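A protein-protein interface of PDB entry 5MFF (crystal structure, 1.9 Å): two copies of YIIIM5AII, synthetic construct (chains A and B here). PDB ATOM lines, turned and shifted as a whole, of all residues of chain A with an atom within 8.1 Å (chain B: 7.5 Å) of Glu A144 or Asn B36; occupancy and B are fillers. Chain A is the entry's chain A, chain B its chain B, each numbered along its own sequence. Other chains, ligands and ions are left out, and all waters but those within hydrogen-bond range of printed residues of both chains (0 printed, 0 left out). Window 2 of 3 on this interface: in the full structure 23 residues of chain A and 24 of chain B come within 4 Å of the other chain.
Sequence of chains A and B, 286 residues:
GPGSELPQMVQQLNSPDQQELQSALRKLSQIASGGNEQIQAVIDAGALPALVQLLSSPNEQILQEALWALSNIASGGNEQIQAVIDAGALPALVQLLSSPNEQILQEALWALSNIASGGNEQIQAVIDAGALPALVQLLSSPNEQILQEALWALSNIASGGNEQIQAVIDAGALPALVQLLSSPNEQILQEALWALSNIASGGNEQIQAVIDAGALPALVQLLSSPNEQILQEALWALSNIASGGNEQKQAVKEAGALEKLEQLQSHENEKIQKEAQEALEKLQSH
The side-chain carboxylate (OE2) of Glu A144 sits at hydrogen-bond distance from the backbone NH (N) of Asn B36 (2.8 Å). NE2 of Gln A145 lies within hydrogen-bond range of O of Ser B33. The side-chain amide nitrogen (NE2) of Gln A145 lies close to the backbone NH (N) of Gly B35, 3.4 Å away. The side-chain amide nitrogen (NE2) of Gln A187 sits at hydrogen-bond distance from the side-chain amide oxygen (OD1) of Asn B78.
The side-chain amide oxygen (OD1) of Asn A143 lies within hydrogen-bond range of the backbone NH (N) of Gln A145 (3.1 Å). The backbone carbonyl oxygen (O) of Glu A144 sits close to the side-chain amide oxygen (OE1) of Gln A148 (3.4 Å). The side-chain amide oxygen (OD1) of Asn A185 sits at hydrogen-bond distance from the backbone NH (N) of Gln A187. The backbone carbonyl oxygen (O) of Gly B34 lies close to the side-chain amide oxygen (OE1) of Gln B38 (3.1 Å). OD1 of Asn B36 is in hydrogen-bond range of N of Gly B77, 3.4 Å away. The backbone carbonyl oxygen (O) of Asn B36 sits at hydrogen-bond distance from the side-chain amide nitrogen (NE2) of Gln B80 (2.8 Å).
Glu A144 touches Gly B35. Gly B34 touches Gln A145. Asn B78 touches Glu A186 (ND2 to OE1, 3.8 Å).
Glu A144 touches two residues of chain B. Of chain A, only Glu A144 comes within 4 Å of Asn B36. Of chain A, only Glu A144 and Gln A145 come within 4 Å of Gly B35. Printed residues of chain B within 4 Å of Glu A186: Asn B78. Printed residues of chain A within 4 Å of Gly B34: Gln A145. Ile B43 touches none of the printed residues of chain A. The nearest residue of chain A that does not touch Asn B36 is Asn A185 (4.1 Å). The nearest printed residue of chain B that does not touch Gln A187 is Gly B77 (4.8 Å).
Of the 21 printed residues of chain B, 5 touch a printed residue of chain A. Printed residues of chain B that touch a printed residue of chain A: Ser B33, Gly B34, Gly B35, Asn B36 and Asn B78. Along chain A the printed residues that touch a printed residue of chain B span positions 144 to 187. Among the printed residues, no Asp or Glu carboxylate lies within 4 Å of a Lys or Arg side-chain nitrogen of the other chain.
No position is printed for both chains.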
ATOM      1  N   GLU A 102     -23.411   3.161   2.998  1.00  0.00           N
ATOM      2  CA  GLU A 102     -23.665   1.906   2.273  1.00  0.00           C
ATOM      3  C   GLU A 102     -23.655   0.654   3.172  1.00  0.00           C
ATOM      4  O   GLU A 102     -24.349  -0.317   2.864  1.00  0.00           O
ATOM      5  CB  GLU A 102     -22.706   1.757   1.085  1.00  0.00           C
ATOM      6  CG  GLU A 102     -23.084   2.652  -0.087  1.00  0.00           C
ATOM      7  CD  GLU A 102     -22.019   2.919  -1.137  1.00  0.00           C
ATOM      8  OE1 GLU A 102     -20.810   2.816  -0.820  1.00  0.00           O
ATOM      9  OE2 GLU A 102     -22.400   3.250  -2.285  1.00  0.00           O
ATOM     10  N   LEU A 138     -33.243   2.696  -5.740  1.00  0.00           N
ATOM     11  CA  LEU A 138     -31.966   1.986  -5.561  1.00  0.00           C
ATOM     12  C   LEU A 138     -31.579   1.120  -6.777  1.00  0.00           C
ATOM     13  O   LEU A 138     -30.434   0.681  -6.869  1.00  0.00           O
ATOM     14  CB  LEU A 138     -31.926   1.162  -4.251  1.00  0.00           C
ATOM     15  CG  LEU A 138     -31.967   1.986  -2.926  1.00  0.00           C
ATOM     16  CD1 LEU A 138     -32.262   1.107  -1.731  1.00  0.00           C
ATOM     17  CD2 LEU A 138     -30.693   2.777  -2.704  1.00  0.00           C
ATOM     18  N   SER A 141     -28.754   2.738  -8.680  1.00  0.00           N
ATOM     19  CA  SER A 141     -27.519   2.857  -7.909  1.00  0.00           C
ATOM     20  C   SER A 141     -26.248   2.416  -8.641  1.00  0.00           C
ATOM     21  O   SER A 141     -26.227   1.333  -9.228  1.00  0.00           O
ATOM     22  CB  SER A 141     -27.648   2.113  -6.585  1.00  0.00           C
ATOM     23  OG  SER A 141     -26.448   2.105  -5.829  1.00  0.00           O
ATOM     24  N   PRO A 142     -25.150   3.211  -8.546  1.00  0.00           N
ATOM     25  CA  PRO A 142     -23.889   2.782  -9.175  1.00  0.00           C
ATOM     26  C   PRO A 142     -23.147   1.724  -8.345  1.00  0.00           C
ATOM     27  O   PRO A 142     -22.224   1.094  -8.863  1.00  0.00           O
ATOM     28  CB  PRO A 142     -23.097   4.088  -9.325  1.00  0.00           C
ATOM     29  CG  PRO A 142     -23.637   4.996  -8.286  1.00  0.00           C
ATOM     30  CD  PRO A 142     -24.995   4.512  -7.853  1.00  0.00           C
ATOM     31  N   ASN A 143     -23.558   1.512  -7.070  1.00  0.00           N
ATOM     32  CA  ASN A 143     -22.959   0.515  -6.182  1.00  0.00           C
ATOM     33  C   ASN A 143     -23.612  -0.861  -6.410  1.00  0.00           C
ATOM     34  O   ASN A 143     -24.763  -1.078  -6.024  1.00  0.00           O
ATOM     35  CB  ASN A 143     -23.069   0.951  -4.714  1.00  0.00           C
ATOM     36  CG  ASN A 143     -22.189   0.143  -3.798  1.00  0.00           C
ATOM     37  OD1 ASN A 143     -22.381  -1.059  -3.610  1.00  0.00           O
ATOM     38  ND2 ASN A 143     -21.166   0.775  -3.248  1.00  0.00           N
ATOM     39  N   GLU A 144     -22.852  -1.793  -7.021  1.00  0.00           N
ATOM     40  CA  GLU A 144     -23.290  -3.146  -7.385  1.00  0.00           C
ATOM     41  C   GLU A 144     -23.719  -4.004  -6.192  1.00  0.00           C
ATOM     42  O   GLU A 144     -24.591  -4.856  -6.341  1.00  0.00           O
ATOM     43  CB  GLU A 144     -22.239  -3.878  -8.260  1.00  0.00           C
ATOM     44  CG  GLU A 144     -20.892  -4.201  -7.621  1.00  0.00           C
ATOM     45  CD  GLU A 144     -20.011  -3.036  -7.207  1.00  0.00           C
ATOM     46  OE1 GLU A 144     -19.822  -2.099  -8.017  1.00  0.00           O
ATOM     47  OE2 GLU A 144     -19.506  -3.064  -6.062  1.00  0.00           O
ATOM     48  N   GLN A 145     -23.133  -3.757  -5.015  1.00  0.00           N
ATOM     49  CA  GLN A 145     -23.426  -4.466  -3.766  1.00  0.00           C
ATOM     50  C   GLN A 145     -24.841  -4.095  -3.275  1.00  0.00           C
ATOM     51  O   GLN A 145     -25.618  -4.977  -2.899  1.00  0.00           O
ATOM     52  CB  GLN A 145     -22.359  -4.098  -2.724  1.00  0.00           C
ATOM     53  CG  GLN A 145     -22.234  -5.070  -1.563  1.00  0.00           C
ATOM     54  CD  GLN A 145     -21.115  -4.663  -0.629  1.00  0.00           C
ATOM     55  OE1 GLN A 145     -21.016  -3.511  -0.189  1.00  0.00           O
ATOM     56  NE2 GLN A 145     -20.258  -5.606  -0.290  1.00  0.00           N
ATOM     57  N   ILE A 146     -25.181  -2.792  -3.330  1.00  0.00           N
ATOM     58  CA  ILE A 146     -26.488  -2.263  -2.937  1.00  0.00           C
ATOM     59  C   ILE A 146     -27.558  -2.681  -3.954  1.00  0.00           C
ATOM     60  O   ILE A 146     -28.662  -3.082  -3.571  1.00  0.00           O
ATOM     61  CB  ILE A 146     -26.401  -0.722  -2.744  1.00  0.00           C
ATOM     62  CG1 ILE A 146     -25.413  -0.322  -1.594  1.00  0.00           C
ATOM     63  CG2 ILE A 146     -27.777  -0.086  -2.568  1.00  0.00           C
ATOM     64  CD1 ILE A 146     -25.618  -1.072  -0.146  1.00  0.00           C
ATOM     65  N   LEU A 147     -27.211  -2.598  -5.253  1.00  0.00           N
ATOM     66  CA  LEU A 147     -28.078  -2.977  -6.354  1.00  0.00           C
ATOM     67  C   LEU A 147     -28.549  -4.440  -6.200  1.00  0.00           C
ATOM     68  O   LEU A 147     -29.752  -4.703  -6.298  1.00  0.00           O
ATOM     69  CB  LEU A 147     -27.331  -2.740  -7.676  1.00  0.00           C
ATOM     70  CG  LEU A 147     -28.099  -2.874  -8.983  1.00  0.00           C
ATOM     71  CD1 LEU A 147     -29.438  -2.172  -8.912  1.00  0.00           C
ATOM     72  CD2 LEU A 147     -27.271  -2.302 -10.144  1.00  0.00           C
ATOM     73  N   GLN A 148     -27.619  -5.355  -5.860  1.00  0.00           N
ATOM     74  CA  GLN A 148     -27.933  -6.769  -5.636  1.00  0.00           C
ATOM     75  C   GLN A 148     -28.871  -6.982  -4.448  1.00  0.00           C
ATOM     76  O   GLN A 148     -29.801  -7.781  -4.551  1.00  0.00           O
ATOM     77  CB  GLN A 148     -26.654  -7.607  -5.488  1.00  0.00           C
ATOM     78  CG  GLN A 148     -26.012  -7.958  -6.838  1.00  0.00           C
ATOM     79  CD  GLN A 148     -24.648  -8.599  -6.697  1.00  0.00           C
ATOM     80  OE1 GLN A 148     -23.617  -8.008  -7.039  1.00  0.00           O
ATOM     81  NE2 GLN A 148     -24.609  -9.830  -6.203  1.00  0.00           N
ATOM     82  N   GLU A 149     -28.638  -6.268  -3.329  1.00  0.00           N
ATOM     83  CA  GLU A 149     -29.498  -6.363  -2.141  1.00  0.00           C
ATOM     84  C   GLU A 149     -30.904  -5.839  -2.452  1.00  0.00           C
ATOM     85  O   GLU A 149     -31.897  -6.465  -2.070  1.00  0.00           O
ATOM     86  CB  GLU A 149     -28.893  -5.607  -0.940  1.00  0.00           C
ATOM     87  CG  GLU A 149     -27.599  -6.204  -0.391  1.00  0.00           C
ATOM     88  CD  GLU A 149     -27.620  -7.618   0.169  1.00  0.00           C
ATOM     89  OE1 GLU A 149     -28.716  -8.143   0.478  1.00  0.00           O
ATOM     90  OE2 GLU A 149     -26.520  -8.194   0.324  1.00  0.00           O
ATOM     91  N   ALA A 150     -30.976  -4.726  -3.195  1.00  0.00           N
ATOM     92  CA  ALA A 150     -32.235  -4.090  -3.589  1.00  0.00           C
ATOM     93  C   ALA A 150     -33.023  -5.020  -4.520  1.00  0.00           C
ATOM     94  O   ALA A 150     -34.223  -5.196  -4.307  1.00  0.00           O
ATOM     95  CB  ALA A 150     -31.965  -2.736  -4.260  1.00  0.00           C
ATOM     96  N   LEU A 151     -32.331  -5.651  -5.513  1.00  0.00           N
ATOM     97  CA  LEU A 151     -32.926  -6.623  -6.433  1.00  0.00           C
ATOM     98  C   LEU A 151     -33.459  -7.849  -5.663  1.00  0.00           C
ATOM     99  O   LEU A 151     -34.583  -8.281  -5.912  1.00  0.00           O
ATOM    100  CB  LEU A 151     -31.925  -7.049  -7.532  1.00  0.00           C
ATOM    101  CG  LEU A 151     -31.732  -6.058  -8.678  1.00  0.00           C
ATOM    102  CD1 LEU A 151     -30.491  -6.368  -9.481  1.00  0.00           C
ATOM    103  CD2 LEU A 151     -32.954  -5.984  -9.554  1.00  0.00           C
ATOM    104  N   SER A 183     -26.804  -5.372 -18.365  1.00  0.00           N
ATOM    105  CA  SER A 183     -25.662  -5.275 -17.455  1.00  0.00           C
ATOM    106  C   SER A 183     -24.504  -6.232 -17.808  1.00  0.00           C
ATOM    107  O   SER A 183     -24.739  -7.427 -18.004  1.00  0.00           O
ATOM    108  CB  SER A 183     -26.091  -5.479 -16.007  1.00  0.00           C
ATOM    109  OG  SER A 183     -24.977  -5.586 -15.136  1.00  0.00           O
ATOM    110  N   ASN A 185     -22.311  -7.054 -15.640  1.00  0.00           N
ATOM    111  CA  ASN A 185     -22.136  -7.755 -14.375  1.00  0.00           C
ATOM    112  C   ASN A 185     -23.122  -8.932 -14.326  1.00  0.00           C
ATOM    113  O   ASN A 185     -24.338  -8.717 -14.275  1.00  0.00           O
ATOM    114  CB  ASN A 185     -22.342  -6.793 -13.195  1.00  0.00           C
ATOM    115  CG  ASN A 185     -22.031  -7.366 -11.828  1.00  0.00           C
ATOM    116  OD1 ASN A 185     -22.354  -8.513 -11.494  1.00  0.00           O
ATOM    117  ND2 ASN A 185     -21.481  -6.539 -10.966  1.00  0.00           N
ATOM    118  N   GLU A 186     -22.587 -10.174 -14.338  1.00  0.00           N
ATOM    119  CA  GLU A 186     -23.387 -11.411 -14.342  1.00  0.00           C
ATOM    120  C   GLU A 186     -24.213 -11.624 -13.075  1.00  0.00           C
ATOM    121  O   GLU A 186     -25.294 -12.205 -13.157  1.00  0.00           O
ATOM    122  CB  GLU A 186     -22.522 -12.653 -14.651  1.00  0.00           C
ATOM    123  CG  GLU A 186     -22.140 -12.749 -16.121  1.00  0.00           C
ATOM    124  CD  GLU A 186     -21.056 -13.749 -16.492  1.00  0.00           C
ATOM    125  OE1 GLU A 186     -20.034 -13.830 -15.771  1.00  0.00           O
ATOM    126  OE2 GLU A 186     -21.214 -14.422 -17.538  1.00  0.00           O
ATOM    127  N   GLN A 187     -23.715 -11.170 -11.915  1.00  0.00           N
ATOM    128  CA  GLN A 187     -24.443 -11.287 -10.642  1.00  0.00           C
ATOM    129  C   GLN A 187     -25.693 -10.383 -10.632  1.00  0.00           C
ATOM    130  O   GLN A 187     -26.775 -10.840 -10.252  1.00  0.00           O
ATOM    131  CB  GLN A 187     -23.527 -11.029  -9.431  1.00  0.00           C
ATOM    132  CG  GLN A 187     -22.376 -12.051  -9.279  1.00  0.00           C
ATOM    133  CD  GLN A 187     -22.831 -13.500  -9.183  1.00  0.00           C
ATOM    134  OE1 GLN A 187     -23.706 -13.864  -8.380  1.00  0.00           O
ATOM    135  NE2 GLN A 187     -22.238 -14.366  -9.999  1.00  0.00           N
ATOM    136  N   ILE A 188     -25.546  -9.134 -11.102  1.00  0.00           N
ATOM    137  CA  ILE A 188     -26.640  -8.168 -11.232  1.00  0.00           C
ATOM    138  C   ILE A 188     -27.680  -8.689 -12.241  1.00  0.00           C
ATOM    139  O   ILE A 188     -28.888  -8.610 -11.981  1.00  0.00           O
ATOM    140  CB  ILE A 188     -26.089  -6.763 -11.627  1.00  0.00           C
ATOM    141  CG1 ILE A 188     -25.391  -6.099 -10.414  1.00  0.00           C
ATOM    142  CG2 ILE A 188     -27.216  -5.847 -12.192  1.00  0.00           C
ATOM    143  CD1 ILE A 188     -24.573  -4.900 -10.765  1.00  0.00           C
ATOM    144  N   GLU A 191     -29.771 -11.463 -10.758  1.00  0.00           N
ATOM    145  CA  GLU A 191     -30.756 -10.942  -9.804  1.00  0.00           C
ATOM    146  C   GLU A 191     -31.907 -10.238 -10.527  1.00  0.00           C
ATOM    147  O   GLU A 191     -33.062 -10.372 -10.101  1.00  0.00           O
ATOM    148  CB  GLU A 191     -30.101 -10.008  -8.769  1.00  0.00           C
ATOM    149  CG  GLU A 191     -29.089 -10.662  -7.832  1.00  0.00           C
ATOM    150  CD  GLU A 191     -29.487 -11.956  -7.139  1.00  0.00           C
ATOM    151  OE1 GLU A 191     -30.690 -12.157  -6.853  1.00  0.00           O
ATOM    152  OE2 GLU A 191     -28.578 -12.772  -6.874  1.00  0.00           O
ATOM    153  N   ILE B  31     -11.993  -3.370   3.788  1.00  0.00           N
ATOM    154  CA  ILE B  31     -12.038  -2.759   2.451  1.00  0.00           C
ATOM    155  C   ILE B  31     -12.713  -3.739   1.457  1.00  0.00           C
ATOM    156  O   ILE B  31     -13.587  -3.331   0.693  1.00  0.00           O
ATOM    157  CB  ILE B  31     -10.645  -2.247   1.998  1.00  0.00           C
ATOM    158  CG1 ILE B  31     -10.255  -1.012   2.839  1.00  0.00           C
ATOM    159  CG2 ILE B  31     -10.618  -1.902   0.496  1.00  0.00           C
ATOM    160  CD1 ILE B  31      -8.844  -0.820   3.054  1.00  0.00           C
ATOM    161  N   ALA B  32     -12.359  -5.033   1.542  1.00  0.00           N
ATOM    162  CA  ALA B  32     -12.904  -6.091   0.692  1.00  0.00           C
ATOM    163  C   ALA B  32     -14.418  -6.358   0.914  1.00  0.00           C
ATOM    164  O   ALA B  32     -15.051  -6.954   0.049  1.00  0.00           O
ATOM    165  CB  ALA B  32     -12.102  -7.375   0.879  1.00  0.00           C
ATOM    166  N   SER B  33     -14.991  -5.912   2.045  1.00  0.00           N
ATOM    167  CA  SER B  33     -16.412  -6.088   2.363  1.00  0.00           C
ATOM    168  C   SER B  33     -17.314  -4.985   1.774  1.00  0.00           C
ATOM    169  O   SER B  33     -18.532  -5.040   1.959  1.00  0.00           O
ATOM    170  CB  SER B  33     -16.612  -6.170   3.873  1.00  0.00           C
ATOM    171  OG  SER B  33     -16.314  -4.931   4.497  1.00  0.00           O
ATOM    172  N   GLY B  34     -16.715  -4.018   1.074  1.00  0.00           N
ATOM    173  CA  GLY B  34     -17.413  -2.861   0.524  1.00  0.00           C
ATOM    174  C   GLY B  34     -17.587  -2.750  -0.978  1.00  0.00           C
ATOM    175  O   GLY B  34     -17.629  -1.633  -1.507  1.00  0.00           O
ATOM    176  N   GLY B  35     -17.720  -3.878  -1.665  1.00  0.00           N
ATOM    177  CA  GLY B  35     -17.975  -3.856  -3.101  1.00  0.00           C
ATOM    178  C   GLY B  35     -16.857  -4.266  -4.031  1.00  0.00           C
ATOM    179  O   GLY B  35     -15.690  -4.323  -3.635  1.00  0.00           O
ATOM    180  N   ASN B  36     -17.237  -4.519  -5.302  1.00  0.00           N
ATOM    181  CA  ASN B  36     -16.385  -4.985  -6.399  1.00  0.00           C
ATOM    182  C   ASN B  36     -15.202  -4.074  -6.713  1.00  0.00           C
ATOM    183  O   ASN B  36     -14.116  -4.590  -6.981  1.00  0.00           O
ATOM    184  CB  ASN B  36     -17.216  -5.240  -7.657  1.00  0.00           C
ATOM    185  CG  ASN B  36     -17.983  -6.554  -7.678  1.00  0.00           C
ATOM    186  OD1 ASN B  36     -18.072  -7.221  -8.715  1.00  0.00           O
ATOM    187  ND2 ASN B  36     -18.578  -6.955  -6.555  1.00  0.00           N
ATOM    188  N   GLU B  37     -15.410  -2.732  -6.702  1.00  0.00           N
ATOM    189  CA  GLU B  37     -14.352  -1.741  -6.968  1.00  0.00           C
ATOM    190  C   GLU B  37     -13.263  -1.819  -5.882  1.00  0.00           C
ATOM    191  O   GLU B  37     -12.076  -1.863  -6.205  1.00  0.00           O
ATOM    192  CB  GLU B  37     -14.945  -0.328  -7.041  1.00  0.00           C
ATOM    193  CG  GLU B  37     -14.099   0.662  -7.824  1.00  0.00           C
ATOM    194  CD  GLU B  37     -14.503   2.122  -7.713  1.00  0.00           C
ATOM    195  OE1 GLU B  37     -15.695   2.396  -7.439  1.00  0.00           O
ATOM    196  OE2 GLU B  37     -13.629   2.997  -7.926  1.00  0.00           O
ATOM    197  N   GLN B  38     -13.687  -1.857  -4.604  1.00  0.00           N
ATOM    198  CA  GLN B  38     -12.826  -1.961  -3.431  1.00  0.00           C
ATOM    199  C   GLN B  38     -12.066  -3.299  -3.407  1.00  0.00           C
ATOM    200  O   GLN B  38     -10.861  -3.288  -3.150  1.00  0.00           O
ATOM    201  CB  GLN B  38     -13.632  -1.737  -2.150  1.00  0.00           C
ATOM    202  CG  GLN B  38     -13.951  -0.262  -1.899  1.00  0.00           C
ATOM    203  CD  GLN B  38     -14.887  -0.015  -0.736  1.00  0.00           C
ATOM    204  OE1 GLN B  38     -15.833   0.775  -0.839  1.00  0.00           O
ATOM    205  NE2 GLN B  38     -14.626  -0.641   0.410  1.00  0.00           N
ATOM    206  N   ILE B  39     -12.751  -4.429  -3.745  1.00  0.00           N
ATOM    207  CA  ILE B  39     -12.164  -5.780  -3.834  1.00  0.00           C
ATOM    208  C   ILE B  39     -11.058  -5.774  -4.903  1.00  0.00           C
ATOM    209  O   ILE B  39      -9.961  -6.268  -4.640  1.00  0.00           O
ATOM    210  CB  ILE B  39     -13.227  -6.899  -4.118  1.00  0.00           C
ATOM    211  CG1 ILE B  39     -14.187  -7.082  -2.931  1.00  0.00           C
ATOM    212  CG2 ILE B  39     -12.547  -8.234  -4.470  1.00  0.00           C
ATOM    213  CD1 ILE B  39     -15.491  -7.903  -3.222  1.00  0.00           C
ATOM    214  N   GLN B  40     -11.367  -5.221  -6.101  1.00  0.00           N
ATOM    215  CA  GLN B  40     -10.439  -5.114  -7.223  1.00  0.00           C
ATOM    216  C   GLN B  40      -9.239  -4.262  -6.838  1.00  0.00           C
ATOM    217  O   GLN B  40      -8.130  -4.593  -7.236  1.00  0.00           O
ATOM    218  CB  GLN B  40     -11.121  -4.542  -8.486  1.00  0.00           C
ATOM    219  CG  GLN B  40     -10.324  -4.780  -9.779  1.00  0.00           C
ATOM    220  CD  GLN B  40     -10.047  -6.245 -10.035  1.00  0.00           C
ATOM    221  OE1 GLN B  40     -10.945  -7.096  -9.995  1.00  0.00           O
ATOM    222  NE2 GLN B  40      -8.789  -6.577 -10.278  1.00  0.00           N
ATOM    223  N   ALA B  41      -9.445  -3.197  -6.037  1.00  0.00           N
ATOM    224  CA  ALA B  41      -8.329  -2.357  -5.583  1.00  0.00           C
ATOM    225  C   ALA B  41      -7.391  -3.215  -4.703  1.00  0.00           C
ATOM    226  O   ALA B  41      -6.175  -3.171  -4.890  1.00  0.00           O
ATOM    227  CB  ALA B  41      -8.844  -1.145  -4.819  1.00  0.00           C
ATOM    228  N   VAL B  42      -7.974  -4.063  -3.817  1.00  0.00           N
ATOM    229  CA  VAL B  42      -7.242  -4.995  -2.949  1.00  0.00           C
ATOM    230  C   VAL B  42      -6.477  -6.016  -3.807  1.00  0.00           C
ATOM    231  O   VAL B  42      -5.301  -6.265  -3.535  1.00  0.00           O
ATOM    232  CB  VAL B  42      -8.170  -5.619  -1.866  1.00  0.00           C
ATOM    233  CG1 VAL B  42      -7.578  -6.883  -1.242  1.00  0.00           C
ATOM    234  CG2 VAL B  42      -8.503  -4.595  -0.787  1.00  0.00           C
ATOM    235  N   ILE B  43      -7.111  -6.538  -4.885  1.00  0.00           N
ATOM    236  CA  ILE B  43      -6.476  -7.482  -5.824  1.00  0.00           C
ATOM    237  C   ILE B  43      -5.290  -6.799  -6.556  1.00  0.00           C
ATOM    238  O   ILE B  43      -4.184  -7.344  -6.578  1.00  0.00           O
ATOM    239  CB  ILE B  43      -7.504  -8.114  -6.816  1.00  0.00           C
ATOM    240  CG1 ILE B  43      -8.535  -9.006  -6.066  1.00  0.00           C
ATOM    241  CG2 ILE B  43      -6.785  -8.918  -7.924  1.00  0.00           C
ATOM    242  CD1 ILE B  43      -9.794  -9.443  -6.877  1.00  0.00           C
ATOM    243  N   ASN B  72     -14.346 -12.485   1.817  1.00  0.00           N
ATOM    244  CA  ASN B  72     -14.883 -11.177   1.401  1.00  0.00           C
ATOM    245  C   ASN B  72     -14.479 -10.873  -0.043  1.00  0.00           C
ATOM    246  O   ASN B  72     -15.304 -10.393  -0.815  1.00  0.00           O
ATOM    247  CB  ASN B  72     -14.421 -10.049   2.326  1.00  0.00           C
ATOM    248  CG  ASN B  72     -15.195  -9.917   3.614  1.00  0.00           C
ATOM    249  OD1 ASN B  72     -14.645  -9.544   4.649  1.00  0.00           O
ATOM    250  ND2 ASN B  72     -16.498 -10.153   3.580  1.00  0.00           N
ATOM    251  N   ILE B  73     -13.211 -11.169  -0.410  1.00  0.00           N
ATOM    252  CA  ILE B  73     -12.716 -11.008  -1.784  1.00  0.00           C
ATOM    253  C   ILE B  73     -13.532 -11.955  -2.696  1.00  0.00           C
ATOM    254  O   ILE B  73     -14.025 -11.518  -3.739  1.00  0.00           O
ATOM    255  CB  ILE B  73     -11.181 -11.240  -1.878  1.00  0.00           C
ATOM    256  CG1 ILE B  73     -10.417 -10.127  -1.113  1.00  0.00           C
ATOM    257  CG2 ILE B  73     -10.708 -11.317  -3.343  1.00  0.00           C
ATOM    258  CD1 ILE B  73      -9.017 -10.398  -0.868  1.00  0.00           C
ATOM    259  N   SER B  75     -16.472 -12.861  -2.337  1.00  0.00           N
ATOM    260  CA  SER B  75     -17.883 -12.473  -2.348  1.00  0.00           C
ATOM    261  C   SER B  75     -18.194 -11.482  -3.515  1.00  0.00           C
ATOM    262  O   SER B  75     -19.347 -11.080  -3.701  1.00  0.00           O
ATOM    263  CB  SER B  75     -18.321 -11.931  -0.988  1.00  0.00           C
ATOM    264  OG  SER B  75     -17.960 -10.576  -0.795  1.00  0.00           O
ATOM    265  N   GLY B  76     -17.168 -11.148  -4.308  1.00  0.00           N
ATOM    266  CA  GLY B  76     -17.295 -10.277  -5.474  1.00  0.00           C
ATOM    267  C   GLY B  76     -17.705 -11.030  -6.727  1.00  0.00           C
ATOM    268  O   GLY B  76     -18.331 -12.090  -6.642  1.00  0.00           O
ATOM    269  N   GLY B  77     -17.353 -10.487  -7.889  1.00  0.00           N
ATOM    270  CA  GLY B  77     -17.672 -11.093  -9.178  1.00  0.00           C
ATOM    271  C   GLY B  77     -16.856 -12.328  -9.500  1.00  0.00           C
ATOM    272  O   GLY B  77     -15.854 -12.617  -8.831  1.00  0.00           O
ATOM    273  N   ASN B  78     -17.272 -13.063 -10.550  1.00  0.00           N
ATOM    274  CA  ASN B  78     -16.606 -14.294 -11.007  1.00  0.00           C
ATOM    275  C   ASN B  78     -15.109 -14.100 -11.339  1.00  0.00           C
ATOM    276  O   ASN B  78     -14.310 -14.999 -11.075  1.00  0.00           O
ATOM    277  CB  ASN B  78     -17.367 -14.928 -12.184  1.00  0.00           C
ATOM    278  CG  ASN B  78     -18.734 -15.500 -11.832  1.00  0.00           C
ATOM    279  OD1 ASN B  78     -19.215 -15.425 -10.689  1.00  0.00           O
ATOM    280  ND2 ASN B  78     -19.400 -16.086 -12.820  1.00  0.00           N
ATOM    281  N   GLU B  79     -14.742 -12.922 -11.877  1.00  0.00           N
ATOM    282  CA  GLU B  79     -13.361 -12.540 -12.203  1.00  0.00           C
ATOM    283  C   GLU B  79     -12.523 -12.377 -10.922  1.00  0.00           C
ATOM    284  O   GLU B  79     -11.358 -12.778 -10.886  1.00  0.00           O
ATOM    285  CB  GLU B  79     -13.302 -11.280 -13.107  1.00  0.00           C
ATOM    286  CG  GLU B  79     -14.019 -10.026 -12.592  1.00  0.00           C
ATOM    287  CD  GLU B  79     -15.539 -10.050 -12.498  1.00  0.00           C
ATOM    288  OE1 GLU B  79     -16.181 -10.791 -13.279  1.00  0.00           O
ATOM    289  OE2 GLU B  79     -16.089  -9.327 -11.635  1.00  0.00           O
ATOM    290  N   GLN B  80     -13.148 -11.824  -9.865  1.00  0.00           N
ATOM    291  CA  GLN B  80     -12.544 -11.634  -8.545  1.00  0.00           C
ATOM    292  C   GLN B  80     -12.374 -12.993  -7.845  1.00  0.00           C
ATOM    293  O   GLN B  80     -11.356 -13.211  -7.184  1.00  0.00           O
ATOM    294  CB  GLN B  80     -13.346 -10.621  -7.714  1.00  0.00           C
ATOM    295  CG  GLN B  80     -13.724  -9.391  -8.537  1.00  0.00           C
ATOM    296  CD  GLN B  80     -14.178  -8.222  -7.716  1.00  0.00           C
ATOM    297  OE1 GLN B  80     -15.251  -8.234  -7.100  1.00  0.00           O
ATOM    298  NE2 GLN B  80     -13.391  -7.159  -7.736  1.00  0.00           N
